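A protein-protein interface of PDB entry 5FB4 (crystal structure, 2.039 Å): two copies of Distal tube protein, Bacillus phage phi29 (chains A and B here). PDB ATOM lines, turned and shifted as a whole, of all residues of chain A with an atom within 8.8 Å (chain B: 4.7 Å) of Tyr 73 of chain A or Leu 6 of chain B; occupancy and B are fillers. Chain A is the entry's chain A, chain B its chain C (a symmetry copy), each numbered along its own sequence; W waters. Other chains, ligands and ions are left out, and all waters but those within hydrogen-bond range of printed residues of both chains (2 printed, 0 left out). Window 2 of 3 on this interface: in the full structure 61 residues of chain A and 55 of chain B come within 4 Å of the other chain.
Of the 13 printed residues of chain B, 6 touch a printed residue of chain A.
Along chain B the printed residues that touch a printed residue of chain A span positions 2 to 85.
Printed residues of chain A that touch a printed residue of chain B: Ile 69, Asp 70, Tyr 73, Ala 75, Val 94, Glu 96, Leu 97 and Phe 99.
Hydrophobic or aromatic side chains of chain A within 4 Å of the printed part of chain B: Ile 69, Tyr 73, Val 94, Leu 97 and Phe 99.
Among the printed residues, 12 pairs touch across the chains.
Among the printed residues, pairs that only touch across the chains: Asp 70 of chain A with Asp 84 of chain B (3.1 Å), Ala 75 of chain A with Tyr 3 of chain B (3.3 Å), Tyr 73 of chain A with Pro 5 of chain B (3.4 Å), Phe 99 of chain A with Leu 6 of chain B (3.4 Å), Tyr 73 of chain A with Tyr 85 of chain B (3.7 Å), Leu 97 of chain A with Tyr 3 of chain B (3.8 Å) and Ile 69 of chain A with Leu 6 of chain B (3.9 Å).
The side-chain amide oxygen (OD1) of Asn 82 of chain B is in hydrogen-bond range of the backbone NH (N) of Asp 84 of chain B, at 2.9 Å.
N of Ile 69 of chain A is in hydrogen-bond range of OG1 of Thr 105 of chain A, 3.1 Å away.
The backbone carbonyl oxygen of Tyr 3 of chain B lies within hydrogen-bond range of the side-chain hydroxyl of Tyr 85 of chain B (2.7 Å).
The backbone carbonyl oxygen (O) of Leu 6 of chain B is in hydrogen-bond range of the backbone NH (N) of Phe 53 of chain B, 2.9 Å away.
OH of Tyr 85 of chain B sits at hydrogen-bond distance from N of Ala 2 of chain B, 2.7 Å away.
Of the printed residues of chain B, Ile 69 of chain A touches Leu 6.
Tyr 73 of chain A touches just these residues of chain B: Ala 2, Tyr 3, Pro 5, Leu 6 and Tyr 85.
Of the printed residues of chain B, Val 94 of chain A touches Tyr 3 (3.4 Å).
Of the printed residues of chain B, Glu 96 of chain A touches Tyr 3 (3.4 Å).
Printed residues of chain A within 4 Å of Tyr 3 of chain B: Tyr 73 (3.1 Å), Ala 75 (3.3 Å), Val 94 (3.4 Å), Glu 96 (3.4 Å) and Leu 97 (3.8 Å).
Pro 5 of chain B touches just one residue of chain A: Tyr 73.
Leu 6 of chain B touches just these residues of chain A: Ile 69, Tyr 73 and Phe 99.
Phe 53 of chain B touches none of the printed residues of chain A.
Of the printed residues of chain A, Tyr 85 of chain B touches Tyr 73 (3.7 Å).
The nearest residue of chain B that does not touch Tyr 73 of chain A is Asn 82 of chain B (4.1 Å).
The nearest residue of chain A that does not touch Leu 6 of chain B is Glu 98 of chain A (5.8 Å).
The nearest printed residue of chain B that does not touch Leu 97 of chain A is Leu 6 of chain B (6.1 Å).
The side-chain hydroxyl of Tyr 3 of chain B is in hydrogen-bond range of the backbone NH of Glu 96 of chain A (3.4 Å).
The side-chain hydroxyl (OH) of Tyr 73 of chain A lies within hydrogen-bond range of the backbone NH (N) of Leu 6 of chain B (3.4 Å).
The backbone NH (N) of Tyr 3 of chain B sits at hydrogen-bond distance from the backbone carbonyl oxygen (O) of Tyr 73 of chain A (3.1 Å).
OH of Tyr 3 of chain B sits at hydrogen-bond distance from O of Val 94 of chain A (3.4 Å).
The backbone carbonyl oxygen of Tyr 73 of chain A is in hydrogen-bond range of the backbone NH of Ala 2 of chain B (3.1 Å).
Water W1 lies within hydrogen-bond range of OD2 of Asp 84 of chain B, ND2 of Asn 82 of chain B and OH of Tyr 73 of chain A.
Water W2 lies within hydrogen-bond range of OH of Tyr 3 of chain B (3.1 Å) and O of Val 94 of chain A (3.3 Å).
No position is printed for both chains.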
ATOM      1  N   ILE A  13      19.326   4.258  11.456  1.00  0.00           N
ATOM      2  CA  ILE A  13      19.786   5.614  11.706  1.00  0.00           C
ATOM      3  C   ILE A  13      18.966   6.550  10.839  1.00  0.00           C
ATOM      4  O   ILE A  13      18.918   6.390   9.614  1.00  0.00           O
ATOM      5  CB  ILE A  13      21.285   5.776  11.391  1.00  0.00           C
ATOM      6  CG1 ILE A  13      22.115   4.797  12.225  1.00  0.00           C
ATOM      7  CG2 ILE A  13      21.752   7.196  11.622  1.00  0.00           C
ATOM      8  CD1 ILE A  13      23.603   4.905  11.948  1.00  0.00           C
ATOM      9  N   LEU A  14      18.330   7.525  11.485  1.00  0.00           N
ATOM     10  CA  LEU A  14      17.367   8.418  10.849  1.00  0.00           C
ATOM     11  C   LEU A  14      17.855   9.846  10.712  1.00  0.00           C
ATOM     12  O   LEU A  14      18.665  10.321  11.509  1.00  0.00           O
ATOM     13  CB  LEU A  14      16.068   8.439  11.658  1.00  0.00           C
ATOM     14  CG  LEU A  14      15.559   7.055  12.045  1.00  0.00           C
ATOM     15  CD1 LEU A  14      14.327   7.156  12.935  1.00  0.00           C
ATOM     16  CD2 LEU A  14      15.254   6.282  10.776  1.00  0.00           C
ATOM     17  N   ALA A  15      17.315  10.540   9.718  1.00  0.00           N
ATOM     18  CA  ALA A  15      17.506  11.973   9.591  1.00  0.00           C
ATOM     19  C   ALA A  15      16.237  12.712  10.043  1.00  0.00           C
ATOM     20  O   ALA A  15      15.172  12.111  10.136  1.00  0.00           O
ATOM     21  CB  ALA A  15      17.856  12.324   8.141  1.00  0.00           C
ATOM     22  N   ASP A  16      16.360  13.996  10.366  1.00  0.00           N
ATOM     23  CA  ASP A  16      15.192  14.863  10.558  1.00  0.00           C
ATOM     24  C   ASP A  16      14.300  14.548  11.764  1.00  0.00           C
ATOM     25  O   ASP A  16      13.082  14.690  11.673  1.00  0.00           O
ATOM     26  CB  ASP A  16      14.300  14.840   9.301  1.00  0.00           C
ATOM     27  CG  ASP A  16      15.078  15.077   8.014  1.00  0.00           C
ATOM     28  OD1 ASP A  16      15.922  16.000   7.988  1.00  0.00           O
ATOM     29  OD2 ASP A  16      14.837  14.341   7.025  1.00  0.00           O
ATOM     30  N   VAL A  45      19.103   7.048   6.990  1.00  0.00           N
ATOM     31  CA  VAL A  45      20.467   7.310   6.566  1.00  0.00           C
ATOM     32  C   VAL A  45      21.240   6.016   6.379  1.00  0.00           C
ATOM     33  O   VAL A  45      22.123   5.916   5.527  1.00  0.00           O
ATOM     34  CB  VAL A  45      21.176   8.196   7.608  1.00  0.00           C
ATOM     35  CG1 VAL A  45      22.623   8.422   7.242  1.00  0.00           C
ATOM     36  CG2 VAL A  45      20.416   9.518   7.763  1.00  0.00           C
ATOM     37  N   LEU A  67      30.892   3.121   7.286  1.00  0.00           N
ATOM     38  CA  LEU A  67      30.587   4.102   6.272  1.00  0.00           C
ATOM     39  C   LEU A  67      31.555   5.253   6.442  1.00  0.00           C
ATOM     40  O   LEU A  67      31.893   5.609   7.576  1.00  0.00           O
ATOM     41  CB  LEU A  67      29.150   4.598   6.433  1.00  0.00           C
ATOM     42  CG  LEU A  67      27.993   3.746   5.919  1.00  0.00           C
ATOM     43  CD1 LEU A  67      26.677   4.475   6.171  1.00  0.00           C
ATOM     44  CD2 LEU A  67      28.160   3.430   4.441  1.00  0.00           C
ATOM     45  N   PRO A  68      31.976   5.864   5.325  1.00  0.00           N
ATOM     46  CA  PRO A  68      32.713   7.118   5.450  1.00  0.00           C
ATOM     47  C   PRO A  68      31.830   8.166   6.112  1.00  0.00           C
ATOM     48  O   PRO A  68      30.605   8.184   5.929  1.00  0.00           O
ATOM     49  CB  PRO A  68      33.057   7.479   4.002  1.00  0.00           C
ATOM     50  CG  PRO A  68      32.047   6.752   3.181  1.00  0.00           C
ATOM     51  CD  PRO A  68      31.788   5.468   3.918  1.00  0.00           C
ATOM     52  N   ILE A  69      32.459   9.032   6.890  1.00  0.00           N
ATOM     53  CA  ILE A  69      31.724   9.973   7.708  1.00  0.00           C
ATOM     54  C   ILE A  69      30.829  10.888   6.876  1.00  0.00           C
ATOM     55  O   ILE A  69      29.807  11.344   7.365  1.00  0.00           O
ATOM     56  CB  ILE A  69      32.684  10.809   8.590  1.00  0.00           C
ATOM     57  CG1 ILE A  69      31.883  11.634   9.600  1.00  0.00           C
ATOM     58  CG2 ILE A  69      33.587  11.690   7.727  1.00  0.00           C
ATOM     59  CD1 ILE A  69      32.698  12.109  10.790  1.00  0.00           C
ATOM     60  N   ASP A  70      31.169  11.135   5.613  1.00  0.00           N
ATOM     61  CA  ASP A  70      30.327  12.043   4.823  1.00  0.00           C
ATOM     62  C   ASP A  70      28.942  11.459   4.541  1.00  0.00           C
ATOM     63  O   ASP A  70      27.984  12.201   4.333  1.00  0.00           O
ATOM     64  CB  ASP A  70      30.999  12.417   3.503  1.00  0.00           C
ATOM     65  CG  ASP A  70      31.115  11.240   2.553  1.00  0.00           C
ATOM     66  OD1 ASP A  70      32.045  10.435   2.747  1.00  0.00           O
ATOM     67  OD2 ASP A  70      30.273  11.111   1.634  1.00  0.00           O
ATOM     68  N   LYS A  71      28.819  10.136   4.596  1.00  0.00           N
ATOM     69  CA  LYS A  71      27.519   9.492   4.393  1.00  0.00           C
ATOM     70  C   LYS A  71      26.604   9.647   5.620  1.00  0.00           C
ATOM     71  O   LYS A  71      25.412   9.337   5.571  1.00  0.00           O
ATOM     72  CB  LYS A  71      27.722   8.005   4.068  1.00  0.00           C
ATOM     73  CG  LYS A  71      28.491   7.772   2.767  1.00  0.00           C
ATOM     74  CD  LYS A  71      27.716   8.318   1.581  1.00  0.00           C
ATOM     75  CE  LYS A  71      28.361   7.931   0.263  1.00  0.00           C
ATOM     76  NZ  LYS A  71      28.407   6.482   0.068  1.00  0.00           N
ATOM     77  N   LEU A  72      27.152  10.164   6.710  1.00  0.00           N
ATOM     78  CA  LEU A  72      26.392  10.254   7.953  1.00  0.00           C
ATOM     79  C   LEU A  72      26.126  11.678   8.424  1.00  0.00           C
ATOM     80  O   LEU A  72      25.639  11.873   9.536  1.00  0.00           O
ATOM     81  CB  LEU A  72      27.124   9.497   9.056  1.00  0.00           C
ATOM     82  CG  LEU A  72      27.179   7.984   8.855  1.00  0.00           C
ATOM     83  CD1 LEU A  72      28.326   7.379   9.646  1.00  0.00           C
ATOM     84  CD2 LEU A  72      25.854   7.394   9.292  1.00  0.00           C
ATOM     85  N   TYR A  73      26.418  12.666   7.587  1.00  0.00           N
ATOM     86  CA  TYR A  73      26.291  14.062   8.005  1.00  0.00           C
ATOM     87  C   TYR A  73      24.867  14.448   8.405  1.00  0.00           C
ATOM     88  O   TYR A  73      24.676  15.391   9.174  1.00  0.00           O
ATOM     89  CB  TYR A  73      26.784  14.991   6.894  1.00  0.00           C
ATOM     90  CG  TYR A  73      28.299  15.041   6.775  1.00  0.00           C
ATOM     91  CD1 TYR A  73      29.114  14.773   7.872  1.00  0.00           C
ATOM     92  CD2 TYR A  73      28.914  15.367   5.566  1.00  0.00           C
ATOM     93  CE1 TYR A  73      30.500  14.812   7.764  1.00  0.00           C
ATOM     94  CE2 TYR A  73      30.301  15.415   5.453  1.00  0.00           C
ATOM     95  CZ  TYR A  73      31.083  15.133   6.552  1.00  0.00           C
ATOM     96  OH  TYR A  73      32.453  15.188   6.442  1.00  0.00           O
ATOM     97  N   SER A  74      23.866  13.712   7.929  1.00  0.00           N
ATOM     98  CA  SER A  74      22.477  14.046   8.270  1.00  0.00           C
ATOM     99  C   SER A  74      21.868  13.155   9.375  1.00  0.00           C
ATOM    100  O   SER A  74      20.659  13.186   9.613  1.00  0.00           O
ATOM    101  CB  SER A  74      21.608  14.000   7.010  1.00  0.00           C
ATOM    102  OG  SER A  74      21.505  12.674   6.533  1.00  0.00           O
ATOM    103  N   ALA A  75      22.700  12.365  10.042  1.00  0.00           N
ATOM    104  CA  ALA A  75      22.237  11.482  11.100  1.00  0.00           C
ATOM    105  C   ALA A  75      21.748  12.291  12.290  1.00  0.00           C
ATOM    106  O   ALA A  75      22.412  13.236  12.704  1.00  0.00           O
ATOM    107  CB  ALA A  75      23.339  10.546  11.534  1.00  0.00           C
ATOM    108  N   SER A  76      20.576  11.946  12.820  1.00  0.00           N
ATOM    109  CA  SER A  76      20.039  12.695  13.960  1.00  0.00           C
ATOM    110  C   SER A  76      19.491  11.778  15.048  1.00  0.00           C
ATOM    111  O   SER A  76      19.362  12.182  16.191  1.00  0.00           O
ATOM    112  CB  SER A  76      18.946  13.666  13.504  1.00  0.00           C
ATOM    113  OG  SER A  76      17.802  12.966  13.070  1.00  0.00           O
ATOM    114  N   VAL A  94      21.307  10.813  18.118  1.00  0.00           N
ATOM    115  CA  VAL A  94      22.694  10.843  17.666  1.00  0.00           C
ATOM    116  C   VAL A  94      23.268  12.171  18.159  1.00  0.00           C
ATOM    117  O   VAL A  94      22.667  13.227  17.945  1.00  0.00           O
ATOM    118  CB  VAL A  94      22.826  10.729  16.132  1.00  0.00           C
ATOM    119  CG1 VAL A  94      24.261  10.997  15.700  1.00  0.00           C
ATOM    120  CG2 VAL A  94      22.358   9.338  15.648  1.00  0.00           C
ATOM    121  N   GLU A  96      26.926  12.904  18.153  1.00  0.00           N
ATOM    122  CA  GLU A  96      28.197  13.272  17.541  1.00  0.00           C
ATOM    123  C   GLU A  96      28.711  12.195  16.588  1.00  0.00           C
ATOM    124  O   GLU A  96      28.422  11.012  16.765  1.00  0.00           O
ATOM    125  CB  GLU A  96      29.229  13.583  18.622  1.00  0.00           C
ATOM    126  CG  GLU A  96      30.556  14.047  18.077  1.00  0.00           C
ATOM    127  CD  GLU A  96      31.313  14.885  19.089  1.00  0.00           C
ATOM    128  OE1 GLU A  96      32.556  14.985  18.984  1.00  0.00           O
ATOM    129  OE2 GLU A  96      30.649  15.461  19.982  1.00  0.00           O
ATOM    130  N   LEU A  97      29.456  12.625  15.570  1.00  0.00           N
ATOM    131  CA  LEU A  97      30.129  11.723  14.646  1.00  0.00           C
ATOM    132  C   LEU A  97      31.623  11.798  14.863  1.00  0.00           C
ATOM    133  O   LEU A  97      32.180  12.884  14.994  1.00  0.00           O
ATOM    134  CB  LEU A  97      29.814  12.083  13.195  1.00  0.00           C
ATOM    135  CG  LEU A  97      28.334  12.232  12.870  1.00  0.00           C
ATOM    136  CD1 LEU A  97      28.179  12.754  11.447  1.00  0.00           C
ATOM    137  CD2 LEU A  97      27.611  10.907  13.076  1.00  0.00           C
ATOM    138  N   GLU A  98      32.275  10.644  14.882  1.00  0.00           N
ATOM    139  CA  GLU A  98      33.710  10.601  15.104  1.00  0.00           C
ATOM    140  C   GLU A  98      34.385   9.785  14.003  1.00  0.00           C
ATOM    141  O   GLU A  98      34.046   8.626  13.774  1.00  0.00           O
ATOM    142  CB  GLU A  98      34.015  10.004  16.485  1.00  0.00           C
ATOM    143  CG  GLU A  98      35.482   9.641  16.717  1.00  0.00           C
ATOM    144  CD  GLU A  98      35.772   9.159  18.140  1.00  0.00           C
ATOM    145  OE1 GLU A  98      34.817   8.876  18.892  1.00  0.00           O
ATOM    146  OE2 GLU A  98      36.964   9.033  18.498  1.00  0.00           O
ATOM    147  N   PHE A  99      35.349  10.408  13.334  1.00  0.00           N
ATOM    148  CA  PHE A  99      36.150   9.770  12.301  1.00  0.00           C
ATOM    149  C   PHE A  99      37.048   8.719  12.938  1.00  0.00           C
ATOM    150  O   PHE A  99      37.795   9.036  13.856  1.00  0.00           O
ATOM    151  CB  PHE A  99      36.989  10.829  11.569  1.00  0.00           C
ATOM    152  CG  PHE A  99      37.869  10.283  10.470  1.00  0.00           C
ATOM    153  CD1 PHE A  99      39.142   9.803  10.749  1.00  0.00           C
ATOM    154  CD2 PHE A  99      37.432  10.285   9.157  1.00  0.00           C
ATOM    155  CE1 PHE A  99      39.957   9.313   9.736  1.00  0.00           C
ATOM    156  CE2 PHE A  99      38.230   9.810   8.141  1.00  0.00           C
ATOM    157  CZ  PHE A  99      39.501   9.317   8.429  1.00  0.00           C
ATOM    158  N   LYS A 100      36.968   7.472  12.478  1.00  0.00           N
ATOM    159  CA  LYS A 100      37.915   6.466  12.925  1.00  0.00           C
ATOM    160  C   LYS A 100      38.950   6.250  11.833  1.00  0.00           C
ATOM    161  O   LYS A 100      40.148   6.401  12.056  1.00  0.00           O
ATOM    162  CB  LYS A 100      37.227   5.148  13.270  1.00  0.00           C
ATOM    163  CG  LYS A 100      38.229   4.079  13.711  1.00  0.00           C
ATOM    164  CD  LYS A 100      37.583   2.721  13.920  1.00  0.00           C
ATOM    165  CE  LYS A 100      38.625   1.688  14.334  1.00  0.00           C
ATOM    166  NZ  LYS A 100      38.087   0.306  14.234  1.00  0.00           N
ATOM    167  N   ASN A 101      38.475   5.896  10.646  1.00  0.00           N
ATOM    168  CA  ASN A 101      39.313   5.908   9.452  1.00  0.00           C
ATOM    169  C   ASN A 101      38.454   6.220   8.236  1.00  0.00           C
ATOM    170  O   ASN A 101      37.261   6.513   8.373  1.00  0.00           O
ATOM    171  CB  ASN A 101      40.075   4.590   9.277  1.00  0.00           C
ATOM    172  CG  ASN A 101      39.162   3.395   9.164  1.00  0.00           C
ATOM    173  OD1 ASN A 101      38.326   3.317   8.264  1.00  0.00           O
ATOM    174  ND2 ASN A 101      39.336   2.438  10.068  1.00  0.00           N
ATOM    175  N   VAL A 104      35.374   3.909   8.217  1.00  0.00           N
ATOM    176  CA  VAL A 104      34.650   3.610   9.455  1.00  0.00           C
ATOM    177  C   VAL A 104      34.411   4.855  10.314  1.00  0.00           C
ATOM    178  O   VAL A 104      35.323   5.652  10.548  1.00  0.00           O
ATOM    179  CB  VAL A 104      35.392   2.548  10.299  1.00  0.00           C
ATOM    180  CG1 VAL A 104      34.645   2.258  11.590  1.00  0.00           C
ATOM    181  CG2 VAL A 104      35.568   1.266   9.499  1.00  0.00           C
ATOM    182  N   THR A 105      33.173   4.995  10.780  1.00  0.00           N
ATOM    183  CA  THR A 105      32.730   6.125  11.590  1.00  0.00           C
ATOM    184  C   THR A 105      32.095   5.652  12.895  1.00  0.00           C
ATOM    185  O   THR A 105      31.338   4.681  12.902  1.00  0.00           O
ATOM    186  CB  THR A 105      31.713   6.997  10.818  1.00  0.00           C
ATOM    187  OG1 THR A 105      32.281   7.403   9.564  1.00  0.00           O
ATOM    188  CG2 THR A 105      31.311   8.234  11.635  1.00  0.00           C
ATOM    189  N   VAL A 107      29.465   6.479  15.590  1.00  0.00           N
ATOM    190  CA  VAL A 107      28.279   7.297  15.778  1.00  0.00           C
ATOM    191  C   VAL A 107      27.928   7.295  17.254  1.00  0.00           C
ATOM    192  O   VAL A 107      27.512   6.280  17.808  1.00  0.00           O
ATOM    193  CB  VAL A 107      27.096   6.790  14.939  1.00  0.00           C
ATOM    194  CG1 VAL A 107      25.846   7.667  15.185  1.00  0.00           C
ATOM    195  CG2 VAL A 107      27.471   6.771  13.457  1.00  0.00           C
ATOM    196  N   ALA B   2      23.635  18.264   8.414  1.00  0.00           N
ATOM    197  CA  ALA B   2      23.395  18.725   9.773  1.00  0.00           C
ATOM    198  C   ALA B   2      24.707  18.911  10.544  1.00  0.00           C
ATOM    199  O   ALA B   2      24.811  19.792  11.402  1.00  0.00           O
ATOM    200  CB  ALA B   2      22.488  17.751  10.502  1.00  0.00           C
ATOM    201  N   TYR B   3      25.687  18.056  10.264  1.00  0.00           N
ATOM    202  CA  TYR B   3      26.986  18.114  10.944  1.00  0.00           C
ATOM    203  C   TYR B   3      28.037  18.839  10.103  1.00  0.00           C
ATOM    204  O   TYR B   3      28.072  18.698   8.882  1.00  0.00           O
ATOM    205  CB  TYR B   3      27.463  16.692  11.302  1.00  0.00           C
ATOM    206  CG  TYR B   3      26.812  16.187  12.575  1.00  0.00           C
ATOM    207  CD1 TYR B   3      27.346  16.510  13.818  1.00  0.00           C
ATOM    208  CD2 TYR B   3      25.639  15.431  12.536  1.00  0.00           C
ATOM    209  CE1 TYR B   3      26.750  16.080  14.987  1.00  0.00           C
ATOM    210  CE2 TYR B   3      25.031  14.993  13.705  1.00  0.00           C
ATOM    211  CZ  TYR B   3      25.591  15.328  14.928  1.00  0.00           C
ATOM    212  OH  TYR B   3      25.006  14.906  16.103  1.00  0.00           O
ATOM    213  N   VAL B   4      28.904  19.601  10.762  1.00  0.00           N
ATOM    214  CA  VAL B   4      29.999  20.274  10.072  1.00  0.00           C
ATOM    215  C   VAL B   4      31.048  19.270   9.578  1.00  0.00           C
ATOM    216  O   VAL B   4      31.529  18.440  10.349  1.00  0.00           O
ATOM    217  CB  VAL B   4      30.677  21.316  10.983  1.00  0.00           C
ATOM    218  CG1 VAL B   4      31.852  21.948  10.268  1.00  0.00           C
ATOM    219  CG2 VAL B   4      29.668  22.368  11.405  1.00  0.00           C
ATOM    220  N   PRO B   5      31.405  19.351   8.282  1.00  0.00           N
ATOM    221  CA  PRO B   5      32.315  18.390   7.644  1.00  0.00           C
ATOM    222  C   PRO B   5      33.735  18.457   8.208  1.00  0.00           C
ATOM    223  O   PRO B   5      34.091  19.438   8.868  1.00  0.00           O
ATOM    224  CB  PRO B   5      32.316  18.820   6.166  1.00  0.00           C
ATOM    225  CG  PRO B   5      31.151  19.706   5.998  1.00  0.00           C
ATOM    226  CD  PRO B   5      30.944  20.376   7.332  1.00  0.00           C
ATOM    227  N   LEU B   6      34.521  17.415   7.941  1.00  0.00           N
ATOM    228  CA  LEU B   6      35.898  17.313   8.418  1.00  0.00           C
ATOM    229  C   LEU B   6      36.916  17.732   7.369  1.00  0.00           C
ATOM    230  O   LEU B   6      38.117  17.681   7.611  1.00  0.00           O
ATOM    231  CB  LEU B   6      36.228  15.880   8.844  1.00  0.00           C
ATOM    232  CG  LEU B   6      35.495  15.240  10.013  1.00  0.00           C
ATOM    233  CD1 LEU B   6      36.131  13.904  10.326  1.00  0.00           C
ATOM    234  CD2 LEU B   6      35.592  16.154  11.204  1.00  0.00           C
ATOM    235  N   SER B   7      36.437  18.118   6.196  1.00  0.00           N
ATOM    236  CA  SER B   7      37.325  18.544   5.131  1.00  0.00           C
ATOM    237  C   SER B   7      36.702  19.714   4.392  1.00  0.00           C
ATOM    238  O   SER B   7      35.481  19.885   4.396  1.00  0.00           O
ATOM    239  CB  SER B   7      37.615  17.384   4.180  1.00  0.00           C
ATOM    240  OG  SER B   7      36.453  17.023   3.459  1.00  0.00           O
ATOM    241  N   GLY B   8      37.541  20.530   3.769  1.00  0.00           N
ATOM    242  CA  GLY B   8      37.052  21.716   3.099  1.00  0.00           C
ATOM    243  C   GLY B   8      37.638  21.923   1.718  1.00  0.00           C
ATOM    244  O   GLY B   8      38.730  21.441   1.402  1.00  0.00           O
ATOM    245  N   THR B  52      42.201  18.912   4.676  1.00  0.00           N
ATOM    246  CA  THR B  52      41.559  18.072   5.683  1.00  0.00           C
ATOM    247  C   THR B  52      41.826  18.667   7.061  1.00  0.00           C
ATOM    248  O   THR B  52      42.963  18.978   7.401  1.00  0.00           O
ATOM    249  CB  THR B  52      42.074  16.610   5.633  1.00  0.00           C
ATOM    250  OG1 THR B  52      41.825  16.052   4.336  1.00  0.00           O
ATOM    251  CG2 THR B  52      41.378  15.760   6.679  1.00  0.00           C
ATOM    252  N   PHE B  53      40.767  18.830   7.847  1.00  0.00           N
ATOM    253  CA  PHE B  53      40.861  19.428   9.175  1.00  0.00           C
ATOM    254  C   PHE B  53      41.374  18.435  10.210  1.00  0.00           C
ATOM    255  O   PHE B  53      41.262  17.223  10.037  1.00  0.00           O
ATOM    256  CB  PHE B  53      39.499  19.973   9.614  1.00  0.00           C
ATOM    257  CG  PHE B  53      38.913  20.968   8.658  1.00  0.00           C
ATOM    258  CD1 PHE B  53      39.705  21.952   8.085  1.00  0.00           C
ATOM    259  CD2 PHE B  53      37.580  20.892   8.296  1.00  0.00           C
ATOM    260  CE1 PHE B  53      39.169  22.858   7.183  1.00  0.00           C
ATOM    261  CE2 PHE B  53      37.038  21.797   7.393  1.00  0.00           C
ATOM    262  CZ  PHE B  53      37.833  22.782   6.839  1.00  0.00           C
ATOM    263  N   PHE B  56      39.080  17.683  15.416  1.00  0.00           N
ATOM    264  CA  PHE B  56      37.642  17.679  15.707  1.00  0.00           C
ATOM    265  C   PHE B  56      37.209  16.889  16.956  1.00  0.00           C
ATOM    266  O   PHE B  56      36.279  17.306  17.653  1.00  0.00           O
ATOM    267  CB  PHE B  56      36.860  17.138  14.504  1.00  0.00           C
ATOM    268  CG  PHE B  56      36.420  18.198  13.526  1.00  0.00           C
ATOM    269  CD1 PHE B  56      37.345  19.021  12.906  1.00  0.00           C
ATOM    270  CD2 PHE B  56      35.073  18.380  13.243  1.00  0.00           C
ATOM    271  CE1 PHE B  56      36.937  19.994  12.002  1.00  0.00           C
ATOM    272  CE2 PHE B  56      34.657  19.353  12.342  1.00  0.00           C
ATOM    273  CZ  PHE B  56      35.591  20.163  11.723  1.00  0.00           C
ATOM    274  N   ASN B  82      32.399  22.304   1.101  1.00  0.00           N
ATOM    275  CA  ASN B  82      32.694  20.884   1.247  1.00  0.00           C
ATOM    276  C   ASN B  82      32.049  20.087   0.131  1.00  0.00           C
ATOM    277  O   ASN B  82      30.911  20.359  -0.248  1.00  0.00           O
ATOM    278  CB  ASN B  82      32.228  20.373   2.613  1.00  0.00           C
ATOM    279  CG  ASN B  82      32.337  18.865   2.745  1.00  0.00           C
ATOM    280  OD1 ASN B  82      31.358  18.152   2.525  1.00  0.00           O
ATOM    281  ND2 ASN B  82      33.525  18.371   3.095  1.00  0.00           N
ATOM    282  N   ASP B  84      30.534  17.486  -0.168  1.00  0.00           N
ATOM    283  CA  ASP B  84      29.247  16.847   0.081  1.00  0.00           C
ATOM    284  C   ASP B  84      28.141  17.806   0.532  1.00  0.00           C
ATOM    285  O   ASP B  84      27.028  17.379   0.827  1.00  0.00           O
ATOM    286  CB  ASP B  84      29.442  15.754   1.126  1.00  0.00           C
ATOM    287  CG  ASP B  84      30.529  14.771   0.727  1.00  0.00           C
ATOM    288  OD1 ASP B  84      30.395  14.139  -0.340  1.00  0.00           O
ATOM    289  OD2 ASP B  84      31.533  14.656   1.458  1.00  0.00           O
ATOM    290  N   TYR B  85      28.452  19.096   0.590  1.00  0.00           N
ATOM    291  CA  TYR B  85      27.477  20.100   1.002  1.00  0.00           C
ATOM    292  C   TYR B  85      27.149  21.088  -0.117  1.00  0.00           C
ATOM    293  O   TYR B  85      26.595  22.165   0.126  1.00  0.00           O
ATOM    294  CB  TYR B  85      27.981  20.848   2.230  1.00  0.00           C
ATOM    295  CG  TYR B  85      27.439  20.305   3.529  1.00  0.00           C
ATOM    296  CD1 TYR B  85      26.203  20.718   4.021  1.00  0.00           C
ATOM    297  CD2 TYR B  85      28.167  19.384   4.269  1.00  0.00           C
ATOM    298  CE1 TYR B  85      25.711  20.228   5.222  1.00  0.00           C
ATOM    299  CE2 TYR B  85      27.687  18.890   5.464  1.00  0.00           C
ATOM    300  CZ  TYR B  85      26.458  19.314   5.936  1.00  0.00           C
ATOM    301  OH  TYR B  85      25.987  18.820   7.126  1.00  0.00           O
HETATM  302  O   HOH W   1      33.047  15.571   3.169  1.00  0.00           O
HETATM  303  O   HOH W   2      22.134  16.024  16.295  1.00  0.00           O
